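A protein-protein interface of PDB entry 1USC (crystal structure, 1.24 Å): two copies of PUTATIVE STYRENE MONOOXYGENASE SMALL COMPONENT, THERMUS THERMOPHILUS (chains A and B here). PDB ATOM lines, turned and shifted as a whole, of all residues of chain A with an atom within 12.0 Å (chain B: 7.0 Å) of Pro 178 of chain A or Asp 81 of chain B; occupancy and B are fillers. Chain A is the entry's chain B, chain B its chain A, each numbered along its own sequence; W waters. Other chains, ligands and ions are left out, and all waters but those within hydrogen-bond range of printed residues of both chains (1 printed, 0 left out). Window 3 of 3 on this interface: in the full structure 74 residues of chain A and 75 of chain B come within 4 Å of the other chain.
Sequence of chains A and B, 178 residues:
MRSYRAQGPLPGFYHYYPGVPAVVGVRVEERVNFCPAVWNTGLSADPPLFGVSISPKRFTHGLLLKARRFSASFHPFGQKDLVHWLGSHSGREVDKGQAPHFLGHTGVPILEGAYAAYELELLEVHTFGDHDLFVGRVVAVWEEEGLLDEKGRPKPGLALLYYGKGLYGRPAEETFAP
The backbone carbonyl oxygen of Tyr 168 of chain B sits at hydrogen-bond distance from the backbone NH of Phe 176 of chain A (2.7 Å).
Of the 7 printed residues of chain A, 5 touch a printed residue of chain B.
Hydrophobic or aromatic side chains of chain A within 4 Å of the printed part of chain B: Phe 176, Ala 177 and Pro 178.
O of His 84 of chain B lies within hydrogen-bond range of OG of Ser 88 of chain B, 2.8 Å away.
OH of Tyr 168 of chain B is in hydrogen-bond range of ND1 of His 84 of chain B (2.8 Å).
Leu 167 of chain B touches Arg 153 of chain A (CD2 to NH2, 3.1 Å).
Thr 175 of chain A touches Leu 167 of chain B (CB to CD1, 3.5 Å).
CA of Thr 175 of chain A touches O of Tyr 168 of chain B, at 3.2 Å.
CE1 of Phe 176 of chain A touches CZ of Phe 77 of chain B, at 3.3 Å.
CB of Phe 176 of chain A touches NZ of Lys 80 of chain B, at 3.0 Å.
CA of Ala 177 of chain A touches O of Gly 166 of chain B, 3.4 Å away.
Pro 178 of chain A touches Lys 80 of chain B (CG to CD, 3.3 Å).
Pro 178 of chain A touches His 84 of chain B (CB to CD2, 3.4 Å).
Pro 178 of chain A touches Gly 166 of chain B (CD to O, 3.5 Å).
Pro 178 of chain A touches Tyr 168 of chain B (CD to CD1, 3.5 Å).
Water W1 lies within hydrogen-bond range of O of Gly 166 of chain B and OXT of Pro 178 of chain A.
No position is printed for both chains.
Printed residues of chain B within 4 Å of Arg 153 of chain A: Leu 167 (3.1 Å).
Printed residues of chain B within 4 Å of Thr 175 of chain A: Leu 167 (3.5 Å) and Tyr 168 (3.2 Å).
Of the printed residues of chain B, Ala 177 of chain A touches Gly 166 (3.4 Å).
Of chain B, only Lys 80 (3.3 Å), Asp 81 (3.8 Å), His 84 (3.4 Å), Gly 166 (3.5 Å) and Tyr 168 (3.5 Å) come within 4 Å of Pro 178 of chain A.
Printed residues of chain A within 4 Å of Phe 77 of chain B: Phe 176.
No residue of chain A comes within 4 Å of Gly 78 of chain B.
Gln 79 of chain B touches none of the printed residues of chain A.
Lys 80 of chain B touches just these residues of chain A: Phe 176 (3.0 Å) and Pro 178 (3.3 Å).
Asp 81 of chain B touches just one residue of chain A: Pro 178 (3.8 Å).
No residue of chain A comes within 4 Å of Leu 82 of chain B.
No residue of chain A comes within 4 Å of Val 83 of chain B.
Trp 85 of chain B touches none of the printed residues of chain A.
Of chain A, only Phe 176, Ala 177 and Pro 178 come within 4 Å of Gly 166 of chain B.
Printed residues of chain A within 4 Å of Leu 167 of chain B: Arg 153, Thr 175 and Phe 176.
Printed residues of chain A within 4 Å of Tyr 168 of chain B: Thr 175, Phe 176 and Pro 178.
The nearest residue of chain B that does not touch Pro 178 of chain A is Leu 167 of chain B (5.5 Å).
The nearest residue of chain A that does not touch Asp 81 of chain B is Ala 177 of chain A (6.2 Å).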
ATOM      1  N   LYS A 151     -18.670  35.048 -23.719  1.00  0.00           N
ATOM      2  CA  LYS A 151     -18.357  35.117 -25.145  1.00  0.00           C
ATOM      3  C   LYS A 151     -19.028  36.260 -25.901  1.00  0.00           C
ATOM      4  O   LYS A 151     -18.978  36.311 -27.129  1.00  0.00           O
ATOM      5  CB  LYS A 151     -18.685  33.776 -25.809  1.00  0.00           C
ATOM      6  CG  LYS A 151     -17.759  32.654 -25.357  1.00  0.00           C
ATOM      7  CD  LYS A 151     -18.133  31.314 -25.959  1.00  0.00           C
ATOM      8  CE  LYS A 151     -17.184  30.225 -25.483  1.00  0.00           C
ATOM      9  NZ  LYS A 151     -17.583  28.882 -25.982  1.00  0.00           N
ATOM     10  N   ARG A 153     -22.355  37.033 -25.778  1.00  0.00           N
ATOM     11  CA  ARG A 153     -23.729  36.724 -26.154  1.00  0.00           C
ATOM     12  C   ARG A 153     -24.660  37.258 -25.079  1.00  0.00           C
ATOM     13  O   ARG A 153     -24.263  37.404 -23.924  1.00  0.00           O
ATOM     14  CB  ARG A 153     -23.932  35.214 -26.274  1.00  0.00           C
ATOM     15  CG  ARG A 153     -23.464  34.607 -27.582  1.00  0.00           C
ATOM     16  CD  ARG A 153     -22.291  33.665 -27.382  1.00  0.00           C
ATOM     17  NE  ARG A 153     -22.471  32.795 -26.224  1.00  0.00           N
ATOM     18  CZ  ARG A 153     -21.870  31.618 -26.075  1.00  0.00           C
ATOM     19  NH1 ARG A 153     -21.056  31.163 -27.016  1.00  0.00           N
ATOM     20  NH2 ARG A 153     -22.067  30.904 -24.976  1.00  0.00           N
ATOM     21  N   GLU A 174     -32.586  28.043 -20.266  1.00  0.00           N
ATOM     22  CA  GLU A 174     -31.832  26.793 -20.284  1.00  0.00           C
ATOM     23  C   GLU A 174     -31.001  26.649 -21.559  1.00  0.00           C
ATOM     24  O   GLU A 174     -31.517  26.808 -22.666  1.00  0.00           O
ATOM     25  CB  GLU A 174     -32.784  25.597 -20.169  1.00  0.00           C
ATOM     26  CG  GLU A 174     -33.667  25.576 -18.922  1.00  0.00           C
ATOM     27  CD  GLU A 174     -34.796  26.593 -18.968  1.00  0.00           C
ATOM     28  OE1 GLU A 174     -34.528  27.803 -18.824  1.00  0.00           O
ATOM     29  OE2 GLU A 174     -35.960  26.177 -19.151  1.00  0.00           O
ATOM     30  N   THR A 175     -29.713  26.351 -21.397  1.00  0.00           N
ATOM     31  CA  THR A 175     -28.814  26.167 -22.536  1.00  0.00           C
ATOM     32  C   THR A 175     -28.197  24.773 -22.474  1.00  0.00           C
ATOM     33  O   THR A 175     -28.014  24.216 -21.391  1.00  0.00           O
ATOM     34  CB  THR A 175     -27.681  27.215 -22.545  1.00  0.00           C
ATOM     35  OG1 THR A 175     -26.938  27.134 -21.323  1.00  0.00           O
ATOM     36  CG2 THR A 175     -28.256  28.614 -22.703  1.00  0.00           C
ATOM     37  N   PHE A 176     -27.874  24.213 -23.637  1.00  0.00           N
ATOM     38  CA  PHE A 176     -27.308  22.870 -23.702  1.00  0.00           C
ATOM     39  C   PHE A 176     -26.095  22.796 -24.626  1.00  0.00           C
ATOM     40  O   PHE A 176     -26.044  23.463 -25.659  1.00  0.00           O
ATOM     41  CB  PHE A 176     -28.377  21.882 -24.182  1.00  0.00           C
ATOM     42  CG  PHE A 176     -29.714  22.050 -23.506  1.00  0.00           C
ATOM     43  CD1 PHE A 176     -30.487  23.187 -23.729  1.00  0.00           C
ATOM     44  CD2 PHE A 176     -30.197  21.076 -22.637  1.00  0.00           C
ATOM     45  CE1 PHE A 176     -31.718  23.353 -23.099  1.00  0.00           C
ATOM     46  CE2 PHE A 176     -31.429  21.232 -22.001  1.00  0.00           C
ATOM     47  CZ  PHE A 176     -32.190  22.374 -22.232  1.00  0.00           C
ATOM     48  N   ALA A 177     -25.121  21.972 -24.253  1.00  0.00           N
ATOM     49  CA  ALA A 177     -23.909  21.808 -25.049  1.00  0.00           C
ATOM     50  C   ALA A 177     -23.662  20.337 -25.377  1.00  0.00           C
ATOM     51  O   ALA A 177     -23.091  19.599 -24.574  1.00  0.00           O
ATOM     52  CB  ALA A 177     -22.712  22.385 -24.301  1.00  0.00           C
ATOM     53  N   PRO A 178     -24.095  19.891 -26.569  1.00  0.00           N
ATOM     54  CA  PRO A 178     -23.925  18.504 -27.014  1.00  0.00           C
ATOM     55  C   PRO A 178     -22.471  18.042 -26.954  1.00  0.00           C
ATOM     56  O   PRO A 178     -22.206  17.021 -26.286  1.00  0.00           O
ATOM     57  CB  PRO A 178     -24.458  18.535 -28.444  1.00  0.00           C
ATOM     58  CG  PRO A 178     -25.509  19.592 -28.382  1.00  0.00           C
ATOM     59  CD  PRO A 178     -24.831  20.673 -27.577  1.00  0.00           C
ATOM     60  OXT PRO A 178     -21.617  18.706 -27.581  1.00  0.00           O
ATOM     61  N   PHE B  77     -36.175  21.338 -31.281  1.00  0.00           N
ATOM     62  CA  PHE B  77     -35.121  21.295 -30.277  1.00  0.00           C
ATOM     63  C   PHE B  77     -34.703  19.852 -29.981  1.00  0.00           C
ATOM     64  O   PHE B  77     -33.545  19.586 -29.655  1.00  0.00           O
ATOM     65  CB  PHE B  77     -35.613  21.965 -28.992  1.00  0.00           C
ATOM     66  CG  PHE B  77     -34.620  21.921 -27.871  1.00  0.00           C
ATOM     67  CD1 PHE B  77     -33.514  22.764 -27.871  1.00  0.00           C
ATOM     68  CD2 PHE B  77     -34.776  21.016 -26.828  1.00  0.00           C
ATOM     69  CE1 PHE B  77     -32.576  22.705 -26.848  1.00  0.00           C
ATOM     70  CE2 PHE B  77     -33.841  20.951 -25.798  1.00  0.00           C
ATOM     71  CZ  PHE B  77     -32.741  21.796 -25.809  1.00  0.00           C
ATOM     72  N   GLY B  78     -35.651  18.929 -30.104  1.00  0.00           N
ATOM     73  CA  GLY B  78     -35.372  17.527 -29.839  1.00  0.00           C
ATOM     74  C   GLY B  78     -34.280  16.921 -30.701  1.00  0.00           C
ATOM     75  O   GLY B  78     -33.722  15.877 -30.352  1.00  0.00           O
ATOM     76  N   GLN B  79     -33.972  17.559 -31.828  1.00  0.00           N
ATOM     77  CA  GLN B  79     -32.929  17.057 -32.716  1.00  0.00           C
ATOM     78  C   GLN B  79     -31.604  17.801 -32.563  1.00  0.00           C
ATOM     79  O   GLN B  79     -30.747  17.753 -33.446  1.00  0.00           O
ATOM     80  CB  GLN B  79     -33.398  17.116 -34.169  1.00  0.00           C
ATOM     81  CG  GLN B  79     -34.438  16.067 -34.498  1.00  0.00           C
ATOM     82  CD  GLN B  79     -34.798  16.048 -35.965  1.00  0.00           C
ATOM     83  OE1 GLN B  79     -35.328  17.023 -36.495  1.00  0.00           O
ATOM     84  NE2 GLN B  79     -34.508  14.936 -36.634  1.00  0.00           N
ATOM     85  N   LYS B  80     -31.438  18.479 -31.434  1.00  0.00           N
ATOM     86  CA  LYS B  80     -30.218  19.225 -31.153  1.00  0.00           C
ATOM     87  C   LYS B  80     -28.946  18.398 -31.364  1.00  0.00           C
ATOM     88  O   LYS B  80     -27.992  18.859 -32.000  1.00  0.00           O
ATOM     89  CB  LYS B  80     -30.261  19.731 -29.711  1.00  0.00           C
ATOM     90  CG  LYS B  80     -28.998  20.432 -29.245  1.00  0.00           C
ATOM     91  CD  LYS B  80     -28.700  20.075 -27.795  1.00  0.00           C
ATOM     92  CE  LYS B  80     -29.924  20.239 -26.908  1.00  0.00           C
ATOM     93  NZ  LYS B  80     -29.715  19.631 -25.565  1.00  0.00           N
ATOM     94  N   ASP B  81     -28.926  17.182 -30.827  1.00  0.00           N
ATOM     95  CA  ASP B  81     -27.749  16.328 -30.947  1.00  0.00           C
ATOM     96  C   ASP B  81     -27.393  15.984 -32.392  1.00  0.00           C
ATOM     97  O   ASP B  81     -26.219  15.999 -32.762  1.00  0.00           O
ATOM     98  CB  ASP B  81     -27.949  15.046 -30.134  1.00  0.00           C
ATOM     99  CG  ASP B  81     -27.953  15.301 -28.635  1.00  0.00           C
ATOM    100  OD1 ASP B  81     -28.295  14.372 -27.872  1.00  0.00           O
ATOM    101  OD2 ASP B  81     -27.609  16.425 -28.216  1.00  0.00           O
ATOM    102  N   LEU B  82     -28.399  15.681 -33.206  1.00  0.00           N
ATOM    103  CA  LEU B  82     -28.158  15.342 -34.606  1.00  0.00           C
ATOM    104  C   LEU B  82     -27.646  16.569 -35.362  1.00  0.00           C
ATOM    105  O   LEU B  82     -26.673  16.492 -36.120  1.00  0.00           O
ATOM    106  CB  LEU B  82     -29.446  14.826 -35.259  1.00  0.00           C
ATOM    107  CG  LEU B  82     -29.404  14.576 -36.771  1.00  0.00           C
ATOM    108  CD1 LEU B  82     -28.319  13.564 -37.106  1.00  0.00           C
ATOM    109  CD2 LEU B  82     -30.765  14.092 -37.245  1.00  0.00           C
ATOM    110  N   VAL B  83     -28.297  17.708 -35.153  1.00  0.00           N
ATOM    111  CA  VAL B  83     -27.874  18.925 -35.824  1.00  0.00           C
ATOM    112  C   VAL B  83     -26.434  19.263 -35.441  1.00  0.00           C
ATOM    113  O   VAL B  83     -25.614  19.587 -36.305  1.00  0.00           O
ATOM    114  CB  VAL B  83     -28.813  20.102 -35.475  1.00  0.00           C
ATOM    115  CG1 VAL B  83     -28.242  21.412 -36.008  1.00  0.00           C
ATOM    116  CG2 VAL B  83     -30.187  19.848 -36.079  1.00  0.00           C
ATOM    117  N   HIS B  84     -26.109  19.164 -34.155  1.00  0.00           N
ATOM    118  CA  HIS B  84     -24.751  19.468 -33.725  1.00  0.00           C
ATOM    119  C   HIS B  84     -23.736  18.504 -34.340  1.00  0.00           C
ATOM    120  O   HIS B  84     -22.642  18.912 -34.738  1.00  0.00           O
ATOM    121  CB  HIS B  84     -24.633  19.426 -32.201  1.00  0.00           C
ATOM    122  CG  HIS B  84     -23.289  19.852 -31.701  1.00  0.00           C
ATOM    123  ND1 HIS B  84     -22.760  21.095 -31.968  1.00  0.00           N
ATOM    124  CD2 HIS B  84     -22.353  19.191 -30.980  1.00  0.00           C
ATOM    125  CE1 HIS B  84     -21.554  21.183 -31.435  1.00  0.00           C
ATOM    126  NE2 HIS B  84     -21.283  20.041 -30.829  1.00  0.00           N
ATOM    127  N   TRP B  85     -24.098  17.227 -34.418  1.00  0.00           N
ATOM    128  CA  TRP B  85     -23.201  16.233 -34.997  1.00  0.00           C
ATOM    129  C   TRP B  85     -22.928  16.581 -36.461  1.00  0.00           C
ATOM    130  O   TRP B  85     -21.786  16.539 -36.920  1.00  0.00           O
ATOM    131  CB  TRP B  85     -23.815  14.832 -34.902  1.00  0.00           C
ATOM    132  CG  TRP B  85     -22.892  13.750 -35.390  1.00  0.00           C
ATOM    133  CD1 TRP B  85     -21.903  13.128 -34.678  1.00  0.00           C
ATOM    134  CD2 TRP B  85     -22.830  13.212 -36.716  1.00  0.00           C
ATOM    135  NE1 TRP B  85     -21.230  12.238 -35.480  1.00  0.00           N
ATOM    136  CE2 TRP B  85     -21.778  12.269 -36.736  1.00  0.00           C
ATOM    137  CE3 TRP B  85     -23.561  13.436 -37.891  1.00  0.00           C
ATOM    138  CZ2 TRP B  85     -21.435  11.549 -37.887  1.00  0.00           C
ATOM    139  CZ3 TRP B  85     -23.221  12.719 -39.038  1.00  0.00           C
ATOM    140  CH2 TRP B  85     -22.166  11.786 -39.026  1.00  0.00           C
ATOM    141  N   LEU B  86     -23.980  16.928 -37.193  1.00  0.00           N
ATOM    142  CA  LEU B  86     -23.829  17.291 -38.597  1.00  0.00           C
ATOM    143  C   LEU B  86     -22.974  18.544 -38.759  1.00  0.00           C
ATOM    144  O   LEU B  86     -22.344  18.745 -39.800  1.00  0.00           O
ATOM    145  CB  LEU B  86     -25.201  17.518 -39.236  1.00  0.00           C
ATOM    146  CG  LEU B  86     -26.096  16.281 -39.351  1.00  0.00           C
ATOM    147  CD1 LEU B  86     -27.498  16.715 -39.728  1.00  0.00           C
ATOM    148  CD2 LEU B  86     -25.532  15.315 -40.396  1.00  0.00           C
ATOM    149  N   GLY B  87     -22.956  19.389 -37.731  1.00  0.00           N
ATOM    150  CA  GLY B  87     -22.162  20.603 -37.793  1.00  0.00           C
ATOM    151  C   GLY B  87     -20.795  20.468 -37.147  1.00  0.00           C
ATOM    152  O   GLY B  87     -20.079  21.460 -37.005  1.00  0.00           O
ATOM    153  N   SER B  88     -20.421  19.249 -36.766  1.00  0.00           N
ATOM    154  CA  SER B  88     -19.128  19.017 -36.123  1.00  0.00           C
ATOM    155  C   SER B  88     -18.287  17.962 -36.836  1.00  0.00           C
ATOM    156  O   SER B  88     -17.220  17.578 -36.355  1.00  0.00           O
ATOM    157  CB  SER B  88     -19.331  18.604 -34.659  1.00  0.00           C
ATOM    158  OG  SER B  88     -20.076  19.573 -33.946  1.00  0.00           O
ATOM    159  N   LEU B 160     -35.090  25.127 -32.616  1.00  0.00           N
ATOM    160  CA  LEU B 160     -33.757  24.919 -32.077  1.00  0.00           C
ATOM    161  C   LEU B 160     -33.021  26.243 -32.275  1.00  0.00           C
ATOM    162  O   LEU B 160     -33.022  26.799 -33.377  1.00  0.00           O
ATOM    163  CB  LEU B 160     -33.039  23.803 -32.845  1.00  0.00           C
ATOM    164  CG  LEU B 160     -31.572  23.559 -32.490  1.00  0.00           C
ATOM    165  CD1 LEU B 160     -31.449  23.119 -31.041  1.00  0.00           C
ATOM    166  CD2 LEU B 160     -31.003  22.500 -33.422  1.00  0.00           C
ATOM    167  N   GLY B 166     -21.014  25.673 -30.062  1.00  0.00           N
ATOM    168  CA  GLY B 166     -21.635  24.481 -29.510  1.00  0.00           C
ATOM    169  C   GLY B 166     -22.697  24.650 -28.439  1.00  0.00           C
ATOM    170  O   GLY B 166     -23.051  23.684 -27.763  1.00  0.00           O
ATOM    171  N   LEU B 167     -23.213  25.862 -28.271  1.00  0.00           N
ATOM    172  CA  LEU B 167     -24.240  26.097 -27.266  1.00  0.00           C
ATOM    173  C   LEU B 167     -25.605  26.237 -27.936  1.00  0.00           C
ATOM    174  O   LEU B 167     -25.756  26.989 -28.897  1.00  0.00           O
ATOM    175  CB  LEU B 167     -23.922  27.358 -26.463  1.00  0.00           C
ATOM    176  CG  LEU B 167     -24.865  27.631 -25.287  1.00  0.00           C
ATOM    177  CD1 LEU B 167     -24.780  26.481 -24.293  1.00  0.00           C
ATOM    178  CD2 LEU B 167     -24.498  28.943 -24.620  1.00  0.00           C
ATOM    179  N   TYR B 168     -26.590  25.505 -27.425  1.00  0.00           N
ATOM    180  CA  TYR B 168     -27.940  25.542 -27.981  1.00  0.00           C
ATOM    181  C   TYR B 168     -28.993  25.851 -26.937  1.00  0.00           C
ATOM    182  O   TYR B 168     -28.756  25.748 -25.733  1.00  0.00           O
ATOM    183  CB  TYR B 168     -28.306  24.206 -28.625  1.00  0.00           C
ATOM    184  CG  TYR B 168     -27.395  23.784 -29.743  1.00  0.00           C
ATOM    185  CD1 TYR B 168     -26.120  23.293 -29.478  1.00  0.00           C
ATOM    186  CD2 TYR B 168     -27.805  23.883 -31.069  1.00  0.00           C
ATOM    187  CE1 TYR B 168     -25.272  22.909 -30.510  1.00  0.00           C
ATOM    188  CE2 TYR B 168     -26.967  23.503 -32.109  1.00  0.00           C
ATOM    189  CZ  TYR B 168     -25.704  23.016 -31.820  1.00  0.00           C
ATOM    190  OH  TYR B 168     -24.871  22.633 -32.839  1.00  0.00           O
HETATM  191  O   HOH W   1     -21.227  21.694 -27.637  1.00  0.00           O
